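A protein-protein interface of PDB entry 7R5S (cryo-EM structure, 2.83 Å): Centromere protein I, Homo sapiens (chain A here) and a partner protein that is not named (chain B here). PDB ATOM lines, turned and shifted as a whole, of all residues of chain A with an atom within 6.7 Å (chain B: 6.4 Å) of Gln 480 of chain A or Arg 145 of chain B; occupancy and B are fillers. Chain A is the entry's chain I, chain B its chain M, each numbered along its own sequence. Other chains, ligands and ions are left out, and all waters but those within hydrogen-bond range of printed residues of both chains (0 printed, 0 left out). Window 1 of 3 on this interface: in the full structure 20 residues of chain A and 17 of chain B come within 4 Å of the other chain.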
ATOM      1  N   TRP A 446      -8.732  23.955   1.165  1.00  0.00           N
ATOM      2  CA  TRP A 446      -7.981  22.718   1.323  1.00  0.00           C
ATOM      3  C   TRP A 446      -7.617  22.486   2.785  1.00  0.00           C
ATOM      4  O   TRP A 446      -7.421  23.427   3.558  1.00  0.00           O
ATOM      5  CB  TRP A 446      -6.714  22.755   0.470  1.00  0.00           C
ATOM      6  CG  TRP A 446      -6.042  21.426   0.323  1.00  0.00           C
ATOM      7  CD1 TRP A 446      -6.646  20.207   0.228  1.00  0.00           C
ATOM      8  CD2 TRP A 446      -4.632  21.181   0.255  1.00  0.00           C
ATOM      9  NE1 TRP A 446      -5.701  19.219   0.105  1.00  0.00           N
ATOM     10  CE2 TRP A 446      -4.456  19.790   0.118  1.00  0.00           C
ATOM     11  CE3 TRP A 446      -3.502  22.003   0.296  1.00  0.00           C
ATOM     12  CZ2 TRP A 446      -3.197  19.203   0.023  1.00  0.00           C
ATOM     13  CZ3 TRP A 446      -2.252  21.418   0.201  1.00  0.00           C
ATOM     14  CH2 TRP A 446      -2.111  20.033   0.066  1.00  0.00           C
ATOM     15  N   ASP A 447      -7.526  21.209   3.160  1.00  0.00           N
ATOM     16  CA  ASP A 447      -7.146  20.832   4.515  1.00  0.00           C
ATOM     17  C   ASP A 447      -5.692  20.395   4.635  1.00  0.00           C
ATOM     18  O   ASP A 447      -5.131  20.470   5.733  1.00  0.00           O
ATOM     19  CB  ASP A 447      -8.051  19.705   5.029  1.00  0.00           C
ATOM     20  CG  ASP A 447      -7.925  18.436   4.212  1.00  0.00           C
ATOM     21  OD1 ASP A 447      -7.752  18.536   2.980  1.00  0.00           O
ATOM     22  OD2 ASP A 447      -7.997  17.338   4.802  1.00  0.00           O
ATOM     23  N   GLY A 448      -5.076  19.943   3.548  1.00  0.00           N
ATOM     24  CA  GLY A 448      -3.680  19.565   3.556  1.00  0.00           C
ATOM     25  C   GLY A 448      -3.392  18.081   3.617  1.00  0.00           C
ATOM     26  O   GLY A 448      -2.233  17.706   3.822  1.00  0.00           O
ATOM     27  N   PHE A 475       0.752  32.159  -1.430  1.00  0.00           N
ATOM     28  CA  PHE A 475       1.736  31.977  -0.369  1.00  0.00           C
ATOM     29  C   PHE A 475       1.163  32.273   1.010  1.00  0.00           C
ATOM     30  O   PHE A 475       1.602  31.672   1.994  1.00  0.00           O
ATOM     31  CB  PHE A 475       2.960  32.850  -0.637  1.00  0.00           C
ATOM     32  CG  PHE A 475       3.810  32.365  -1.776  1.00  0.00           C
ATOM     33  CD1 PHE A 475       4.549  31.200  -1.656  1.00  0.00           C
ATOM     34  CD2 PHE A 475       3.868  33.070  -2.965  1.00  0.00           C
ATOM     35  CE1 PHE A 475       5.330  30.749  -2.701  1.00  0.00           C
ATOM     36  CE2 PHE A 475       4.649  32.624  -4.014  1.00  0.00           C
ATOM     37  CZ  PHE A 475       5.380  31.461  -3.882  1.00  0.00           C
ATOM     38  N   ASP A 476       0.184  33.174   1.110  1.00  0.00           N
ATOM     39  CA  ASP A 476      -0.436  33.435   2.405  1.00  0.00           C
ATOM     40  C   ASP A 476      -1.144  32.192   2.931  1.00  0.00           C
ATOM     41  O   ASP A 476      -0.946  31.788   4.084  1.00  0.00           O
ATOM     42  CB  ASP A 476      -1.409  34.609   2.297  1.00  0.00           C
ATOM     43  CG  ASP A 476      -0.700  35.948   2.239  1.00  0.00           C
ATOM     44  OD1 ASP A 476       0.449  36.034   2.716  1.00  0.00           O
ATOM     45  OD2 ASP A 476      -1.296  36.915   1.721  1.00  0.00           O
ATOM     46  N   HIS A 477      -1.970  31.565   2.089  1.00  0.00           N
ATOM     47  CA  HIS A 477      -2.645  30.338   2.494  1.00  0.00           C
ATOM     48  C   HIS A 477      -1.644  29.214   2.729  1.00  0.00           C
ATOM     49  O   HIS A 477      -1.809  28.410   3.657  1.00  0.00           O
ATOM     50  CB  HIS A 477      -3.674  29.932   1.439  1.00  0.00           C
ATOM     51  CG  HIS A 477      -4.625  31.027   1.071  1.00  0.00           C
ATOM     52  ND1 HIS A 477      -5.593  31.494   1.934  1.00  0.00           N
ATOM     53  CD2 HIS A 477      -4.757  31.748  -0.068  1.00  0.00           C
ATOM     54  CE1 HIS A 477      -6.280  32.455   1.343  1.00  0.00           C
ATOM     55  NE2 HIS A 477      -5.793  32.628   0.127  1.00  0.00           N
ATOM     56  N   LEU A 478      -0.596  29.143   1.903  1.00  0.00           N
ATOM     57  CA  LEU A 478       0.422  28.116   2.102  1.00  0.00           C
ATOM     58  C   LEU A 478       1.100  28.266   3.459  1.00  0.00           C
ATOM     59  O   LEU A 478       1.300  27.277   4.168  1.00  0.00           O
ATOM     60  CB  LEU A 478       1.455  28.168   0.977  1.00  0.00           C
ATOM     61  CG  LEU A 478       1.134  27.336  -0.266  1.00  0.00           C
ATOM     62  CD1 LEU A 478       2.263  27.428  -1.279  1.00  0.00           C
ATOM     63  CD2 LEU A 478       0.871  25.888   0.114  1.00  0.00           C
ATOM     64  N   ALA A 479       1.438  29.496   3.848  1.00  0.00           N
ATOM     65  CA  ALA A 479       2.083  29.713   5.139  1.00  0.00           C
ATOM     66  C   ALA A 479       1.121  29.450   6.291  1.00  0.00           C
ATOM     67  O   ALA A 479       1.519  28.900   7.325  1.00  0.00           O
ATOM     68  CB  ALA A 479       2.637  31.134   5.218  1.00  0.00           C
ATOM     69  N   GLN A 480      -0.147  29.840   6.133  1.00  0.00           N
ATOM     70  CA  GLN A 480      -1.123  29.596   7.191  1.00  0.00           C
ATOM     71  C   GLN A 480      -1.342  28.105   7.406  1.00  0.00           C
ATOM     72  O   GLN A 480      -1.551  27.657   8.540  1.00  0.00           O
ATOM     73  CB  GLN A 480      -2.442  30.295   6.858  1.00  0.00           C
ATOM     74  CG  GLN A 480      -3.485  30.204   7.959  1.00  0.00           C
ATOM     75  CD  GLN A 480      -4.671  31.114   7.715  1.00  0.00           C
ATOM     76  OE1 GLN A 480      -4.587  32.068   6.941  1.00  0.00           O
ATOM     77  NE2 GLN A 480      -5.786  30.824   8.374  1.00  0.00           N
ATOM     78  N   LEU A 481      -1.294  27.316   6.330  1.00  0.00           N
ATOM     79  CA  LEU A 481      -1.384  25.867   6.459  1.00  0.00           C
ATOM     80  C   LEU A 481      -0.065  25.238   6.895  1.00  0.00           C
ATOM     81  O   LEU A 481      -0.069  24.131   7.442  1.00  0.00           O
ATOM     82  CB  LEU A 481      -1.838  25.255   5.132  1.00  0.00           C
ATOM     83  CG  LEU A 481      -2.571  23.915   5.181  1.00  0.00           C
ATOM     84  CD1 LEU A 481      -3.852  24.040   5.982  1.00  0.00           C
ATOM     85  CD2 LEU A 481      -2.865  23.427   3.774  1.00  0.00           C
ATOM     86  N   PHE A 482       1.053  25.927   6.665  1.00  0.00           N
ATOM     87  CA  PHE A 482       2.377  25.410   6.987  1.00  0.00           C
ATOM     88  C   PHE A 482       2.697  25.556   8.469  1.00  0.00           C
ATOM     89  O   PHE A 482       3.261  24.640   9.078  1.00  0.00           O
ATOM     90  CB  PHE A 482       3.412  26.137   6.122  1.00  0.00           C
ATOM     91  CG  PHE A 482       4.835  25.979   6.577  1.00  0.00           C
ATOM     92  CD1 PHE A 482       5.410  26.895   7.444  1.00  0.00           C
ATOM     93  CD2 PHE A 482       5.613  24.941   6.101  1.00  0.00           C
ATOM     94  CE1 PHE A 482       6.722  26.757   7.850  1.00  0.00           C
ATOM     95  CE2 PHE A 482       6.928  24.803   6.499  1.00  0.00           C
ATOM     96  CZ  PHE A 482       7.481  25.710   7.375  1.00  0.00           C
ATOM     97  N   PHE A 483       2.346  26.694   9.065  1.00  0.00           N
ATOM     98  CA  PHE A 483       2.708  26.977  10.448  1.00  0.00           C
ATOM     99  C   PHE A 483       1.886  26.196  11.466  1.00  0.00           C
ATOM    100  O   PHE A 483       2.170  26.292  12.664  1.00  0.00           O
ATOM    101  CB  PHE A 483       2.574  28.476  10.726  1.00  0.00           C
ATOM    102  CG  PHE A 483       3.712  29.294  10.190  1.00  0.00           C
ATOM    103  CD1 PHE A 483       5.017  28.852  10.314  1.00  0.00           C
ATOM    104  CD2 PHE A 483       3.475  30.501   9.554  1.00  0.00           C
ATOM    105  CE1 PHE A 483       6.066  29.600   9.820  1.00  0.00           C
ATOM    106  CE2 PHE A 483       4.521  31.253   9.056  1.00  0.00           C
ATOM    107  CZ  PHE A 483       5.818  30.802   9.191  1.00  0.00           C
ATOM    108  N   THR A 484       0.881  25.430  11.033  1.00  0.00           N
ATOM    109  CA  THR A 484       0.022  24.700  11.958  1.00  0.00           C
ATOM    110  C   THR A 484      -0.075  23.213  11.636  1.00  0.00           C
ATOM    111  O   THR A 484      -0.905  22.518  12.233  1.00  0.00           O
ATOM    112  CB  THR A 484      -1.387  25.309  11.980  1.00  0.00           C
ATOM    113  OG1 THR A 484      -1.935  25.302  10.657  1.00  0.00           O
ATOM    114  CG2 THR A 484      -1.345  26.738  12.498  1.00  0.00           C
ATOM    115  N   SER A 485       0.743  22.706  10.722  1.00  0.00           N
ATOM    116  CA  SER A 485       0.701  21.310  10.310  1.00  0.00           C
ATOM    117  C   SER A 485       1.894  20.554  10.889  1.00  0.00           C
ATOM    118  O   SER A 485       2.688  21.092  11.665  1.00  0.00           O
ATOM    119  CB  SER A 485       0.667  21.203   8.785  1.00  0.00           C
ATOM    120  OG  SER A 485      -0.543  21.727   8.266  1.00  0.00           O
ATOM    121  N   TYR A 539      11.740  34.820   1.437  1.00  0.00           N
ATOM    122  CA  TYR A 539      10.512  34.322   2.045  1.00  0.00           C
ATOM    123  C   TYR A 539      10.679  32.886   2.527  1.00  0.00           C
ATOM    124  O   TYR A 539      10.275  32.539   3.644  1.00  0.00           O
ATOM    125  CB  TYR A 539       9.365  34.431   1.039  1.00  0.00           C
ATOM    126  CG  TYR A 539       8.023  33.971   1.556  1.00  0.00           C
ATOM    127  CD1 TYR A 539       7.276  34.772   2.407  1.00  0.00           C
ATOM    128  CD2 TYR A 539       7.496  32.744   1.178  1.00  0.00           C
ATOM    129  CE1 TYR A 539       6.045  34.359   2.877  1.00  0.00           C
ATOM    130  CE2 TYR A 539       6.266  32.324   1.642  1.00  0.00           C
ATOM    131  CZ  TYR A 539       5.547  33.135   2.491  1.00  0.00           C
ATOM    132  OH  TYR A 539       4.322  32.721   2.957  1.00  0.00           O
ATOM    133  N   PRO B 127      -7.454  35.272  12.447  1.00  0.00           N
ATOM    134  CA  PRO B 127      -7.444  34.326  11.326  1.00  0.00           C
ATOM    135  C   PRO B 127      -8.826  33.752  11.059  1.00  0.00           C
ATOM    136  O   PRO B 127      -9.735  33.816  11.890  1.00  0.00           O
ATOM    137  CB  PRO B 127      -6.473  33.232  11.790  1.00  0.00           C
ATOM    138  CG  PRO B 127      -5.705  33.838  12.924  1.00  0.00           C
ATOM    139  CD  PRO B 127      -6.646  34.792  13.578  1.00  0.00           C
ATOM    140  N   LEU B 128      -8.973  33.178   9.867  1.00  0.00           N
ATOM    141  CA  LEU B 128     -10.221  32.564   9.430  1.00  0.00           C
ATOM    142  C   LEU B 128      -9.915  31.182   8.877  1.00  0.00           C
ATOM    143  O   LEU B 128      -9.086  31.045   7.971  1.00  0.00           O
ATOM    144  CB  LEU B 128     -10.921  33.425   8.374  1.00  0.00           C
ATOM    145  CG  LEU B 128     -12.231  32.878   7.807  1.00  0.00           C
ATOM    146  CD1 LEU B 128     -13.281  32.754   8.898  1.00  0.00           C
ATOM    147  CD2 LEU B 128     -12.733  33.756   6.672  1.00  0.00           C
ATOM    148  N   LEU B 129     -10.582  30.166   9.415  1.00  0.00           N
ATOM    149  CA  LEU B 129     -10.376  28.785   9.010  1.00  0.00           C
ATOM    150  C   LEU B 129     -11.636  28.231   8.357  1.00  0.00           C
ATOM    151  O   LEU B 129     -12.755  28.639   8.682  1.00  0.00           O
ATOM    152  CB  LEU B 129      -9.988  27.915  10.209  1.00  0.00           C
ATOM    153  CG  LEU B 129      -8.830  28.422  11.071  1.00  0.00           C
ATOM    154  CD1 LEU B 129      -8.576  27.482  12.237  1.00  0.00           C
ATOM    155  CD2 LEU B 129      -7.573  28.592  10.235  1.00  0.00           C
ATOM    156  N   TYR B 130     -11.442  27.295   7.433  1.00  0.00           N
ATOM    157  CA  TYR B 130     -12.534  26.640   6.726  1.00  0.00           C
ATOM    158  C   TYR B 130     -12.471  25.140   6.969  1.00  0.00           C
ATOM    159  O   TYR B 130     -11.400  24.531   6.875  1.00  0.00           O
ATOM    160  CB  TYR B 130     -12.471  26.920   5.220  1.00  0.00           C
ATOM    161  CG  TYR B 130     -12.854  28.328   4.829  1.00  0.00           C
ATOM    162  CD1 TYR B 130     -14.185  28.687   4.669  1.00  0.00           C
ATOM    163  CD2 TYR B 130     -11.883  29.295   4.607  1.00  0.00           C
ATOM    164  CE1 TYR B 130     -14.539  29.972   4.307  1.00  0.00           C
ATOM    165  CE2 TYR B 130     -12.228  30.582   4.245  1.00  0.00           C
ATOM    166  CZ  TYR B 130     -13.557  30.915   4.095  1.00  0.00           C
ATOM    167  OH  TYR B 130     -13.905  32.195   3.734  1.00  0.00           O
ATOM    168  N   ALA B 140     -10.695  15.652  11.896  1.00  0.00           N
ATOM    169  CA  ALA B 140      -9.506  15.218  12.624  1.00  0.00           C
ATOM    170  C   ALA B 140      -8.330  16.156  12.371  1.00  0.00           C
ATOM    171  O   ALA B 140      -7.621  16.556  13.306  1.00  0.00           O
ATOM    172  CB  ALA B 140      -9.149  13.784  12.235  1.00  0.00           C
ATOM    173  N   THR B 141      -8.110  16.524  11.106  1.00  0.00           N
ATOM    174  CA  THR B 141      -7.017  17.434  10.778  1.00  0.00           C
ATOM    175  C   THR B 141      -7.244  18.809  11.394  1.00  0.00           C
ATOM    176  O   THR B 141      -6.307  19.426  11.922  1.00  0.00           O
ATOM    177  CB  THR B 141      -6.866  17.544   9.261  1.00  0.00           C
ATOM    178  OG1 THR B 141      -6.749  16.233   8.695  1.00  0.00           O
ATOM    179  CG2 THR B 141      -5.628  18.351   8.905  1.00  0.00           C
ATOM    180  N   MET B 142      -8.483  19.307  11.337  1.00  0.00           N
ATOM    181  CA  MET B 142      -8.780  20.594  11.955  1.00  0.00           C
ATOM    182  C   MET B 142      -8.555  20.545  13.462  1.00  0.00           C
ATOM    183  O   MET B 142      -8.047  21.505  14.054  1.00  0.00           O
ATOM    184  CB  MET B 142     -10.215  21.013  11.636  1.00  0.00           C
ATOM    185  CG  MET B 142     -10.618  22.351  12.233  1.00  0.00           C
ATOM    186  SD  MET B 142      -9.477  23.682  11.811  1.00  0.00           S
ATOM    187  CE  MET B 142      -9.615  23.699  10.026  1.00  0.00           C
ATOM    188  N   ALA B 143      -8.912  19.426  14.096  1.00  0.00           N
ATOM    189  CA  ALA B 143      -8.696  19.283  15.532  1.00  0.00           C
ATOM    190  C   ALA B 143      -7.212  19.277  15.868  1.00  0.00           C
ATOM    191  O   ALA B 143      -6.791  19.887  16.857  1.00  0.00           O
ATOM    192  CB  ALA B 143      -9.366  18.005  16.034  1.00  0.00           C
ATOM    193  N   GLN B 144      -6.401  18.595  15.056  1.00  0.00           N
ATOM    194  CA  GLN B 144      -4.960  18.591  15.301  1.00  0.00           C
ATOM    195  C   GLN B 144      -4.369  19.988  15.145  1.00  0.00           C
ATOM    196  O   GLN B 144      -3.533  20.415  15.955  1.00  0.00           O
ATOM    197  CB  GLN B 144      -4.269  17.604  14.360  1.00  0.00           C
ATOM    198  CG  GLN B 144      -4.680  16.160  14.576  1.00  0.00           C
ATOM    199  CD  GLN B 144      -4.541  15.727  16.022  1.00  0.00           C
ATOM    200  OE1 GLN B 144      -3.501  15.935  16.647  1.00  0.00           O
ATOM    201  NE2 GLN B 144      -5.595  15.127  16.563  1.00  0.00           N
ATOM    202  N   ARG B 145      -4.795  20.718  14.110  1.00  0.00           N
ATOM    203  CA  ARG B 145      -4.318  22.088  13.932  1.00  0.00           C
ATOM    204  C   ARG B 145      -4.717  22.970  15.111  1.00  0.00           C
ATOM    205  O   ARG B 145      -3.912  23.777  15.595  1.00  0.00           O
ATOM    206  CB  ARG B 145      -4.857  22.665  12.624  1.00  0.00           C
ATOM    207  CG  ARG B 145      -4.324  21.982  11.377  1.00  0.00           C
ATOM    208  CD  ARG B 145      -4.994  22.527  10.128  1.00  0.00           C
ATOM    209  NE  ARG B 145      -4.772  23.961   9.971  1.00  0.00           N
ATOM    210  CZ  ARG B 145      -5.401  24.720   9.080  1.00  0.00           C
ATOM    211  NH1 ARG B 145      -6.297  24.184   8.263  1.00  0.00           N
ATOM    212  NH2 ARG B 145      -5.136  26.017   9.007  1.00  0.00           N
ATOM    213  N   LEU B 146      -5.956  22.828  15.589  1.00  0.00           N
ATOM    214  CA  LEU B 146      -6.402  23.621  16.731  1.00  0.00           C
ATOM    215  C   LEU B 146      -5.620  23.267  17.989  1.00  0.00           C
ATOM    216  O   LEU B 146      -5.314  24.142  18.803  1.00  0.00           O
ATOM    217  CB  LEU B 146      -7.901  23.425  16.955  1.00  0.00           C
ATOM    218  CG  LEU B 146      -8.831  24.092  15.941  1.00  0.00           C
ATOM    219  CD1 LEU B 146     -10.284  23.848  16.306  1.00  0.00           C
ATOM    220  CD2 LEU B 146      -8.540  25.580  15.847  1.00  0.00           C
ATOM    221  N   VAL B 147      -5.285  21.986  18.164  1.00  0.00           N
ATOM    222  CA  VAL B 147      -4.495  21.579  19.325  1.00  0.00           C
ATOM    223  C   VAL B 147      -3.104  22.196  19.263  1.00  0.00           C
ATOM    224  O   VAL B 147      -2.567  22.660  20.277  1.00  0.00           O
ATOM    225  CB  VAL B 147      -4.435  20.043  19.420  1.00  0.00           C
ATOM    226  CG1 VAL B 147      -3.327  19.606  20.364  1.00  0.00           C
ATOM    227  CG2 VAL B 147      -5.772  19.492  19.885  1.00  0.00           C
ATOM    228  N   ARG B 148      -2.500  22.222  18.072  1.00  0.00           N
ATOM    229  CA  ARG B 148      -1.187  22.849  17.937  1.00  0.00           C
ATOM    230  C   ARG B 148      -1.254  24.345  18.229  1.00  0.00           C
ATOM    231  O   ARG B 148      -0.381  24.894  18.916  1.00  0.00           O
ATOM    232  CB  ARG B 148      -0.621  22.599  16.540  1.00  0.00           C
ATOM    233  CG  ARG B 148      -0.375  21.133  16.228  1.00  0.00           C
ATOM    234  CD  ARG B 148       0.478  20.968  14.983  1.00  0.00           C
ATOM    235  NE  ARG B 148       1.864  21.362  15.212  1.00  0.00           N
ATOM    236  CZ  ARG B 148       2.818  20.530  15.618  1.00  0.00           C
ATOM    237  NH1 ARG B 148       2.536  19.254  15.840  1.00  0.00           N
ATOM    238  NH2 ARG B 148       4.054  20.974  15.803  1.00  0.00           N
ATOM    239  N   VAL B 149      -2.289  25.021  17.721  1.00  0.00           N
ATOM    240  CA  VAL B 149      -2.439  26.452  17.985  1.00  0.00           C
ATOM    241  C   VAL B 149      -2.642  26.705  19.475  1.00  0.00           C
ATOM    242  O   VAL B 149      -2.108  27.670  20.037  1.00  0.00           O
ATOM    243  CB  VAL B 149      -3.593  27.033  17.147  1.00  0.00           C
ATOM    244  CG1 VAL B 149      -3.868  28.475  17.540  1.00  0.00           C
ATOM    245  CG2 VAL B 149      -3.267  26.943  15.666  1.00  0.00           C
ATOM    246  N   LEU B 150      -3.410  25.838  20.142  1.00  0.00           N
ATOM    247  CA  LEU B 150      -3.625  25.985  21.578  1.00  0.00           C
ATOM    248  C   LEU B 150      -2.330  25.782  22.353  1.00  0.00           C
ATOM    249  O   LEU B 150      -2.057  26.509  23.316  1.00  0.00           O
ATOM    250  CB  LEU B 150      -4.692  24.999  22.052  1.00  0.00           C
ATOM    251  CG  LEU B 150      -4.861  24.858  23.566  1.00  0.00           C
ATOM    252  CD1 LEU B 150      -5.314  26.172  24.182  1.00  0.00           C
ATOM    253  CD2 LEU B 150      -5.835  23.740  23.897  1.00  0.00           C
ATOM    254  N   LEU B 168       2.636  35.735  12.469  1.00  0.00           N
ATOM    255  CA  LEU B 168       2.872  34.603  11.577  1.00  0.00           C
ATOM    256  C   LEU B 168       1.679  34.359  10.659  1.00  0.00           C
ATOM    257  O   LEU B 168       1.855  33.987   9.493  1.00  0.00           O
ATOM    258  CB  LEU B 168       3.186  33.348  12.390  1.00  0.00           C
ATOM    259  CG  LEU B 168       4.514  33.338  13.147  1.00  0.00           C
ATOM    260  CD1 LEU B 168       4.713  32.011  13.861  1.00  0.00           C
ATOM    261  CD2 LEU B 168       5.667  33.621  12.202  1.00  0.00           C
ATOM    262  N   LEU B 169       0.462  34.563  11.163  1.00  0.00           N
ATOM    263  CA  LEU B 169      -0.754  34.300  10.407  1.00  0.00           C
ATOM    264  C   LEU B 169      -1.350  35.564   9.796  1.00  0.00           C
ATOM    265  O   LEU B 169      -2.542  35.584   9.470  1.00  0.00           O
ATOM    266  CB  LEU B 169      -1.787  33.608  11.299  1.00  0.00           C
ATOM    267  CG  LEU B 169      -1.331  32.324  11.992  1.00  0.00           C
ATOM    268  CD1 LEU B 169      -2.455  31.735  12.829  1.00  0.00           C
ATOM    269  CD2 LEU B 169      -0.828  31.313  10.976  1.00  0.00           C
ATOM    270  N   SER B 171      -2.304  38.358   7.057  1.00  0.00           N
ATOM    271  CA  SER B 171      -2.595  38.355   5.631  1.00  0.00           C
ATOM    272  C   SER B 171      -2.063  39.623   4.976  1.00  0.00           C
ATOM    273  O   SER B 171      -1.995  40.686   5.598  1.00  0.00           O
ATOM    274  CB  SER B 171      -4.100  38.233   5.387  1.00  0.00           C
ATOM    275  OG  SER B 171      -4.597  36.999   5.875  1.00  0.00           O
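NE2 of Gln 480 of chain A is in hydrogen-bond range of O of Leu 128 of chain B (3.3 Å).
NE of Arg 145 of chain B lies within hydrogen-bond range of OG1 of Thr 484 of chain A (3.2 Å).
The side-chain hydroxyl (OG1) of Thr 484 of chain A lies within hydrogen-bond range of the backbone carbonyl oxygen (O) of Gln 480 of chain A.
The side-chain hydroxyl (OG) of Ser 485 of chain A lies within hydrogen-bond range of the backbone carbonyl oxygen (O) of Leu 481 of chain A.
Among the printed residues, pairs that only touch across the chains: Leu 481 of chain A with Arg 145 of chain B (3.3 Å), Gln 480 of chain A with Leu 129 of chain B (3.4 Å), Thr 484 of chain A with Arg 148 of chain B (3.4 Å), Ser 485 of chain A with Arg 148 of chain B (3.7 Å), Thr 484 of chain A with Val 149 of chain B (3.7 Å), Phe 483 of chain A with Leu 168 of chain B (3.8 Å), Asp 447 of chain A with Thr 141 of chain B (3.8 Å) and Gln 480 of chain A with Arg 145 of chain B (3.97 Å).
Gln 480 of chain A touches just these residues of chain B: Leu 128 (3.3 Å), Leu 129 (3.4 Å) and Arg 145 (3.97 Å).
Pro 127 of chain B touches none of the printed residues of chain A.
Of chain A, only Gln 480, Leu 481 and Thr 484 come within 4 Å of Arg 145 of chain B.
Printed residues of chain A within 4 Å of Arg 148 of chain B: Thr 484 (3.4 Å) and Ser 485 (3.7 Å).
Of the printed residues of chain A, Leu 168 of chain B touches Phe 483 (3.8 Å).
The nearest residue of chain B that does not touch Gln 480 of chain A is Leu 169 of chain B (4.2 Å).
The nearest residue of chain A that does not touch Arg 145 of chain B is Asp 447 of chain A (4.6 Å).
The nearest printed residue of chain A that does not touch Leu 128 of chain B is His 477 of chain A (7.0 Å).
Hydrophobic or aromatic side chains of chain B within 4 Å of the printed part of chain A: Leu 129 and Val 149.
Hydrophobic or aromatic side chains of chain A that line the printed part of chain B: Leu 481 and Phe 483.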
